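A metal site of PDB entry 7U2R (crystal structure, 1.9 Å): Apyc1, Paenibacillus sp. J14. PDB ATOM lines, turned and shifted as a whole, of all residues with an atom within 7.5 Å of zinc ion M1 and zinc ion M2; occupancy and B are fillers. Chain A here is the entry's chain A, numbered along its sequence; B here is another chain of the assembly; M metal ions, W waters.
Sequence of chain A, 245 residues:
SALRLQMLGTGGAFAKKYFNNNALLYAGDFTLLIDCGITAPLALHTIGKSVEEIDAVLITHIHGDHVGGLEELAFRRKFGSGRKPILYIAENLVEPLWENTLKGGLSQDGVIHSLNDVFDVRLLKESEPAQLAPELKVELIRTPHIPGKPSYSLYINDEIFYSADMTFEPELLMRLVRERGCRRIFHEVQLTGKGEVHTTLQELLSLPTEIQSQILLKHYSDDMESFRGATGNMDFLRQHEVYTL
Water W1 is bound to zinc ion M2. Zinc ion M2 is bound by a ring nitrogen (NE2) of His 66 (2.2 Å). NE2 of His 219 is bound to zinc ion M2, at 2.2 Å. Zinc ion M2 is bound by OD2 of Asp 165, 2.3 Å away. Zinc ion M2 is bound by OD2 of Asp 65 (2.3 Å).
ND1 of His 63 binds zinc ion M1 (2.1 Å). NE2 of His 145 is bound to zinc ion M1 (2.2 Å). Zinc ion M1 is bound by a ring nitrogen (NE2) of His 61, 2.2 Å away. Zinc ion M1 is bound by OD2 of Asp 165 (2.4 Å). Zinc ion M1 is bound by water W1, 2.5 Å away. Zinc ion M1 has five donor atoms within binding distance.
Four residues have an atom within 4 Å of zinc ion M2: Asp 65, His 66, Asp 165 and His 219.
Of the 25 residues printed, 4 come within 4 Å of zinc ion M1. The nearest printed residue that does not touch zinc ion M1 is His 66 (4.2 Å).
ND1 of His 145 is in hydrogen-bond range of O of Val 197, 2.7 Å away. ND1 of His 66 is in hydrogen-bond range of OD2 of Asp 35 (2.7 Å). The backbone carbonyl oxygen of His 219 lies close to the backbone NH of Gly 12. The backbone NH of His 219 is in hydrogen-bond range of the side-chain amide oxygen of Asn 21 (3.0 Å). A ring nitrogen (ND1) of His 61 is in hydrogen-bond range of the side-chain hydroxyl (OG1) of Thr 60. O of Asp 65 sits at hydrogen-bond distance from ND2 of Asn 22.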
ATOM      1  N   GLY A  11      15.731 -13.519  24.950  1.00  0.00           N
ATOM      2  CA  GLY A  11      16.719 -13.573  26.008  1.00  0.00           C
ATOM      3  C   GLY A  11      16.994 -14.978  26.527  1.00  0.00           C
ATOM      4  O   GLY A  11      16.191 -15.877  26.356  1.00  0.00           O
ATOM      5  N   GLY A  12      18.158 -15.148  27.132  1.00  0.00           N
ATOM      6  CA  GLY A  12      18.441 -16.361  27.876  1.00  0.00           C
ATOM      7  C   GLY A  12      17.563 -16.403  29.122  1.00  0.00           C
ATOM      8  O   GLY A  12      16.803 -15.470  29.416  1.00  0.00           O
ATOM      9  N   ALA A  13      17.707 -17.488  29.885  1.00  0.00           N
ATOM     10  CA  ALA A  13      16.758 -17.769  30.974  1.00  0.00           C
ATOM     11  C   ALA A  13      16.696 -16.654  32.013  1.00  0.00           C
ATOM     12  O   ALA A  13      15.635 -16.412  32.601  1.00  0.00           O
ATOM     13  CB  ALA A  13      17.136 -19.084  31.685  1.00  0.00           C
ATOM     14  N   ASN A  20      11.753 -14.163  27.834  1.00  0.00           N
ATOM     15  CA  ASN A  20      12.188 -15.534  27.584  1.00  0.00           C
ATOM     16  C   ASN A  20      12.135 -15.838  26.080  1.00  0.00           C
ATOM     17  O   ASN A  20      11.316 -15.285  25.349  1.00  0.00           O
ATOM     18  CB  ASN A  20      11.276 -16.577  28.269  1.00  0.00           C
ATOM     19  CG  ASN A  20      11.254 -16.527  29.774  1.00  0.00           C
ATOM     20  OD1 ASN A  20      10.311 -17.066  30.374  1.00  0.00           O
ATOM     21  ND2 ASN A  20      12.259 -15.945  30.422  1.00  0.00           N
ATOM     22  N   ASN A  21      12.969 -16.761  25.635  1.00  0.00           N
ATOM     23  CA  ASN A  21      13.168 -17.012  24.198  1.00  0.00           C
ATOM     24  C   ASN A  21      12.035 -17.882  23.661  1.00  0.00           C
ATOM     25  O   ASN A  21      12.099 -19.123  23.657  1.00  0.00           O
ATOM     26  CB  ASN A  21      14.531 -17.658  23.976  1.00  0.00           C
ATOM     27  CG  ASN A  21      14.993 -17.539  22.568  1.00  0.00           C
ATOM     28  OD1 ASN A  21      15.291 -16.449  22.112  1.00  0.00           O
ATOM     29  ND2 ASN A  21      15.055 -18.671  21.863  1.00  0.00           N
ATOM     30  N   ASN A  22      10.959 -17.230  23.234  1.00  0.00           N
ATOM     31  CA  ASN A  22       9.751 -17.917  22.808  1.00  0.00           C
ATOM     32  C   ASN A  22       9.332 -17.272  21.497  1.00  0.00           C
ATOM     33  O   ASN A  22       9.411 -16.048  21.362  1.00  0.00           O
ATOM     34  CB  ASN A  22       8.558 -17.776  23.822  1.00  0.00           C
ATOM     35  CG  ASN A  22       8.892 -18.156  25.281  1.00  0.00           C
ATOM     36  OD1 ASN A  22       8.226 -17.649  26.184  1.00  0.00           O
ATOM     37  ND2 ASN A  22       9.852 -19.065  25.511  1.00  0.00           N
ATOM     38  N   ASP A  35       7.335 -22.563  22.574  1.00  0.00           N
ATOM     39  CA  ASP A  35       7.689 -22.366  23.972  1.00  0.00           C
ATOM     40  C   ASP A  35       6.920 -21.217  24.614  1.00  0.00           C
ATOM     41  O   ASP A  35       6.436 -20.298  23.942  1.00  0.00           O
ATOM     42  CB  ASP A  35       9.205 -22.209  24.141  1.00  0.00           C
ATOM     43  CG  ASP A  35       9.940 -23.527  23.823  1.00  0.00           C
ATOM     44  OD1 ASP A  35       9.281 -24.591  23.979  1.00  0.00           O
ATOM     45  OD2 ASP A  35      11.154 -23.532  23.496  1.00  0.00           O
ATOM     46  N   THR A  60       9.663 -27.445  23.326  1.00  0.00           N
ATOM     47  CA  THR A  60      10.941 -28.036  22.931  1.00  0.00           C
ATOM     48  C   THR A  60      11.627 -28.798  24.041  1.00  0.00           C
ATOM     49  O   THR A  60      12.341 -29.771  23.746  1.00  0.00           O
ATOM     50  CB  THR A  60      11.914 -26.962  22.415  1.00  0.00           C
ATOM     51  OG1 THR A  60      12.334 -26.121  23.500  1.00  0.00           O
ATOM     52  CG2 THR A  60      11.260 -26.123  21.305  1.00  0.00           C
ATOM     53  N   HIS A  61      11.454 -28.395  25.302  1.00  0.00           N
ATOM     54  CA  HIS A  61      12.035 -29.082  26.470  1.00  0.00           C
ATOM     55  C   HIS A  61      11.459 -28.438  27.727  1.00  0.00           C
ATOM     56  O   HIS A  61      10.758 -27.422  27.665  1.00  0.00           O
ATOM     57  CB  HIS A  61      13.575 -29.010  26.490  1.00  0.00           C
ATOM     58  CG  HIS A  61      14.112 -27.635  26.681  1.00  0.00           C
ATOM     59  ND1 HIS A  61      13.909 -26.635  25.758  1.00  0.00           N
ATOM     60  CD2 HIS A  61      14.831 -27.074  27.686  1.00  0.00           C
ATOM     61  CE1 HIS A  61      14.481 -25.519  26.170  1.00  0.00           C
ATOM     62  NE2 HIS A  61      15.024 -25.748  27.348  1.00  0.00           N
ATOM     63  N   ILE A  62      11.809 -29.021  28.877  1.00  0.00           N
ATOM     64  CA  ILE A  62      11.197 -28.638  30.151  1.00  0.00           C
ATOM     65  C   ILE A  62      12.175 -27.779  30.945  1.00  0.00           C
ATOM     66  O   ILE A  62      13.123 -28.281  31.556  1.00  0.00           O
ATOM     67  CB  ILE A  62      10.751 -29.856  30.955  1.00  0.00           C
ATOM     68  CG1 ILE A  62       9.725 -30.637  30.137  1.00  0.00           C
ATOM     69  CG2 ILE A  62      10.137 -29.389  32.259  1.00  0.00           C
ATOM     70  CD1 ILE A  62       9.325 -31.888  30.781  1.00  0.00           C
ATOM     71  N   HIS A  63      11.918 -26.474  30.965  1.00  0.00           N
ATOM     72  CA  HIS A  63      12.639 -25.478  31.738  1.00  0.00           C
ATOM     73  C   HIS A  63      11.685 -24.318  31.898  1.00  0.00           C
ATOM     74  O   HIS A  63      10.861 -24.074  31.011  1.00  0.00           O
ATOM     75  CB  HIS A  63      13.879 -24.951  31.028  1.00  0.00           C
ATOM     76  CG  HIS A  63      15.159 -25.588  31.428  1.00  0.00           C
ATOM     77  ND1 HIS A  63      16.253 -25.556  30.599  1.00  0.00           N
ATOM     78  CD2 HIS A  63      15.549 -26.241  32.558  1.00  0.00           C
ATOM     79  CE1 HIS A  63      17.255 -26.218  31.177  1.00  0.00           C
ATOM     80  NE2 HIS A  63      16.865 -26.606  32.376  1.00  0.00           N
ATOM     81  N   GLY A  64      11.822 -23.576  32.993  1.00  0.00           N
ATOM     82  CA  GLY A  64      10.861 -22.539  33.276  1.00  0.00           C
ATOM     83  C   GLY A  64      10.769 -21.492  32.186  1.00  0.00           C
ATOM     84  O   GLY A  64       9.687 -20.921  31.967  1.00  0.00           O
ATOM     85  N   ASP A  65      11.886 -21.196  31.512  1.00  0.00           N
ATOM     86  CA  ASP A  65      11.786 -20.164  30.477  1.00  0.00           C
ATOM     87  C   ASP A  65      11.158 -20.696  29.189  1.00  0.00           C
ATOM     88  O   ASP A  65      11.046 -19.938  28.217  1.00  0.00           O
ATOM     89  CB  ASP A  65      13.168 -19.526  30.201  1.00  0.00           C
ATOM     90  CG  ASP A  65      14.280 -20.537  29.930  1.00  0.00           C
ATOM     91  OD1 ASP A  65      14.363 -21.569  30.635  1.00  0.00           O
ATOM     92  OD2 ASP A  65      15.093 -20.227  29.054  1.00  0.00           O
ATOM     93  N   HIS A  66      10.729 -21.967  29.184  1.00  0.00           N
ATOM     94  CA  HIS A  66      10.007 -22.549  28.067  1.00  0.00           C
ATOM     95  C   HIS A  66       8.670 -23.161  28.428  1.00  0.00           C
ATOM     96  O   HIS A  66       7.857 -23.374  27.511  1.00  0.00           O
ATOM     97  CB  HIS A  66      10.882 -23.645  27.388  1.00  0.00           C
ATOM     98  CG  HIS A  66      12.202 -23.092  26.966  1.00  0.00           C
ATOM     99  ND1 HIS A  66      12.441 -22.643  25.690  1.00  0.00           N
ATOM    100  CD2 HIS A  66      13.295 -22.767  27.686  1.00  0.00           C
ATOM    101  CE1 HIS A  66      13.662 -22.146  25.619  1.00  0.00           C
ATOM    102  NE2 HIS A  66      14.194 -22.219  26.817  1.00  0.00           N
ATOM    103  N   HIS A 145      21.096 -30.778  25.396  1.00  0.00           N
ATOM    104  CA  HIS A 145      21.016 -29.580  26.229  1.00  0.00           C
ATOM    105  C   HIS A 145      21.325 -30.001  27.663  1.00  0.00           C
ATOM    106  O   HIS A 145      22.465 -29.824  28.116  1.00  0.00           O
ATOM    107  CB  HIS A 145      19.627 -28.935  26.031  1.00  0.00           C
ATOM    108  CG  HIS A 145      19.313 -27.786  26.939  1.00  0.00           C
ATOM    109  ND1 HIS A 145      20.246 -26.819  27.290  1.00  0.00           N
ATOM    110  CD2 HIS A 145      18.152 -27.401  27.520  1.00  0.00           C
ATOM    111  CE1 HIS A 145      19.678 -25.917  28.067  1.00  0.00           C
ATOM    112  NE2 HIS A 145      18.425 -26.267  28.255  1.00  0.00           N
ATOM    113  N   ILE A 146      20.384 -30.573  28.397  1.00  0.00           N
ATOM    114  CA  ILE A 146      20.644 -31.087  29.738  1.00  0.00           C
ATOM    115  C   ILE A 146      20.875 -32.594  29.634  1.00  0.00           C
ATOM    116  O   ILE A 146      20.022 -33.301  29.065  1.00  0.00           O
ATOM    117  CB  ILE A 146      19.497 -30.778  30.715  1.00  0.00           C
ATOM    118  CG1 ILE A 146      19.172 -29.274  30.733  1.00  0.00           C
ATOM    119  CG2 ILE A 146      19.925 -31.239  32.112  1.00  0.00           C
ATOM    120  CD1 ILE A 146      20.369 -28.442  31.229  1.00  0.00           C
ATOM    121  N   SER A 151      15.471 -33.038  24.815  1.00  0.00           N
ATOM    122  CA  SER A 151      15.196 -31.698  24.333  1.00  0.00           C
ATOM    123  C   SER A 151      15.297 -31.728  22.825  1.00  0.00           C
ATOM    124  O   SER A 151      15.945 -32.614  22.256  1.00  0.00           O
ATOM    125  CB  SER A 151      16.164 -30.680  24.959  1.00  0.00           C
ATOM    126  OG  SER A 151      17.504 -30.979  24.643  1.00  0.00           O
ATOM    127  N   ALA A 164      16.431 -23.935  19.171  1.00  0.00           N
ATOM    128  CA  ALA A 164      15.954 -23.920  20.560  1.00  0.00           C
ATOM    129  C   ALA A 164      17.201 -24.010  21.453  1.00  0.00           C
ATOM    130  O   ALA A 164      18.256 -23.465  21.104  1.00  0.00           O
ATOM    131  CB  ALA A 164      14.902 -25.019  20.751  1.00  0.00           C
ATOM    132  N   ASP A 165      17.132 -24.649  22.623  1.00  0.00           N
ATOM    133  CA  ASP A 165      18.280 -24.692  23.528  1.00  0.00           C
ATOM    134  C   ASP A 165      19.119 -25.915  23.177  1.00  0.00           C
ATOM    135  O   ASP A 165      18.588 -27.022  23.138  1.00  0.00           O
ATOM    136  CB  ASP A 165      17.860 -24.817  24.995  1.00  0.00           C
ATOM    137  CG  ASP A 165      17.209 -23.579  25.562  1.00  0.00           C
ATOM    138  OD1 ASP A 165      16.759 -22.730  24.767  1.00  0.00           O
ATOM    139  OD2 ASP A 165      17.113 -23.574  26.814  1.00  0.00           O
ATOM    140  N   MET A 166      20.431 -25.723  22.964  1.00  0.00           N
ATOM    141  CA  MET A 166      21.315 -26.877  22.702  1.00  0.00           C
ATOM    142  C   MET A 166      22.794 -26.508  22.790  1.00  0.00           C
ATOM    143  O   MET A 166      23.164 -25.331  22.649  1.00  0.00           O
ATOM    144  CB  MET A 166      21.037 -27.496  21.336  1.00  0.00           C
ATOM    145  CG  MET A 166      21.417 -26.650  20.130  1.00  0.00           C
ATOM    146  SD  MET A 166      21.149 -27.679  18.455  1.00  0.00           S
ATOM    147  CE  MET A 166      22.820 -27.323  17.507  1.00  0.00           C
ATOM    148  N   GLU A 188      20.626 -20.365  19.301  1.00  0.00           N
ATOM    149  CA  GLU A 188      20.879 -19.841  20.631  1.00  0.00           C
ATOM    150  C   GLU A 188      22.370 -19.544  20.809  1.00  0.00           C
ATOM    151  O   GLU A 188      23.238 -20.106  20.117  1.00  0.00           O
ATOM    152  CB  GLU A 188      20.401 -20.840  21.690  1.00  0.00           C
ATOM    153  CG  GLU A 188      21.199 -22.183  21.740  1.00  0.00           C
ATOM    154  CD  GLU A 188      21.790 -22.365  23.114  1.00  0.00           C
ATOM    155  OE1 GLU A 188      22.824 -21.701  23.434  1.00  0.00           O
ATOM    156  OE2 GLU A 188      21.194 -23.126  23.911  1.00  0.00           O
ATOM    157  N   VAL A 197      25.767 -26.140  28.858  1.00  0.00           N
ATOM    158  CA  VAL A 197      24.476 -26.634  28.405  1.00  0.00           C
ATOM    159  C   VAL A 197      23.895 -25.745  27.301  1.00  0.00           C
ATOM    160  O   VAL A 197      22.782 -25.976  26.855  1.00  0.00           O
ATOM    161  CB  VAL A 197      23.485 -26.761  29.581  1.00  0.00           C
ATOM    162  CG1 VAL A 197      23.968 -27.816  30.588  1.00  0.00           C
ATOM    163  CG2 VAL A 197      23.222 -25.374  30.233  1.00  0.00           C
ATOM    164  N   HIS A 198      24.708 -24.798  26.811  1.00  0.00           N
ATOM    165  CA  HIS A 198      24.379 -23.886  25.720  1.00  0.00           C
ATOM    166  C   HIS A 198      25.555 -23.798  24.762  1.00  0.00           C
ATOM    167  O   HIS A 198      26.658 -24.297  25.037  1.00  0.00           O
ATOM    168  CB  HIS A 198      24.026 -22.477  26.268  1.00  0.00           C
ATOM    169  CG  HIS A 198      22.754 -22.471  27.063  1.00  0.00           C
ATOM    170  ND1 HIS A 198      21.534 -22.720  26.483  1.00  0.00           N
ATOM    171  CD2 HIS A 198      22.530 -22.282  28.386  1.00  0.00           C
ATOM    172  CE1 HIS A 198      20.599 -22.682  27.404  1.00  0.00           C
ATOM    173  NE2 HIS A 198      21.161 -22.410  28.572  1.00  0.00           N
ATOM    174  N   HIS A 219      18.295 -16.241  22.382  1.00  0.00           N
ATOM    175  CA  HIS A 219      18.484 -16.794  23.726  1.00  0.00           C
ATOM    176  C   HIS A 219      19.688 -16.156  24.422  1.00  0.00           C
ATOM    177  O   HIS A 219      20.454 -16.827  25.115  1.00  0.00           O
ATOM    178  CB  HIS A 219      18.622 -18.327  23.657  1.00  0.00           C
ATOM    179  CG  HIS A 219      18.288 -19.038  24.937  1.00  0.00           C
ATOM    180  ND1 HIS A 219      19.214 -19.255  25.937  1.00  0.00           N
ATOM    181  CD2 HIS A 219      17.152 -19.648  25.334  1.00  0.00           C
ATOM    182  CE1 HIS A 219      18.643 -19.924  26.923  1.00  0.00           C
ATOM    183  NE2 HIS A 219      17.389 -20.179  26.575  1.00  0.00           N
ATOM    184  N   GLU B  71      12.084 -21.675  40.150  1.00  0.00           N
ATOM    185  CA  GLU B  71      13.128 -22.317  39.372  1.00  0.00           C
ATOM    186  C   GLU B  71      14.228 -21.326  39.035  1.00  0.00           C
ATOM    187  O   GLU B  71      15.428 -21.635  39.190  1.00  0.00           O
ATOM    188  CB  GLU B  71      12.562 -22.954  38.094  1.00  0.00           C
ATOM    189  CG  GLU B  71      13.666 -23.506  37.193  1.00  0.00           C
ATOM    190  CD  GLU B  71      13.145 -24.136  35.911  1.00  0.00           C
ATOM    191  OE1 GLU B  71      12.226 -24.966  35.969  1.00  0.00           O
ATOM    192  OE2 GLU B  71      13.646 -23.781  34.820  1.00  0.00           O
HETATM  193 ZN    ZN M   1      16.674 -25.002  28.667  1.00  0.00          ZN
HETATM  194 ZN    ZN M   2      16.160 -21.685  27.645  1.00  0.00          ZN
HETATM  195  O   HOH W   1      17.246 -22.635  29.302  1.00  0.00           O
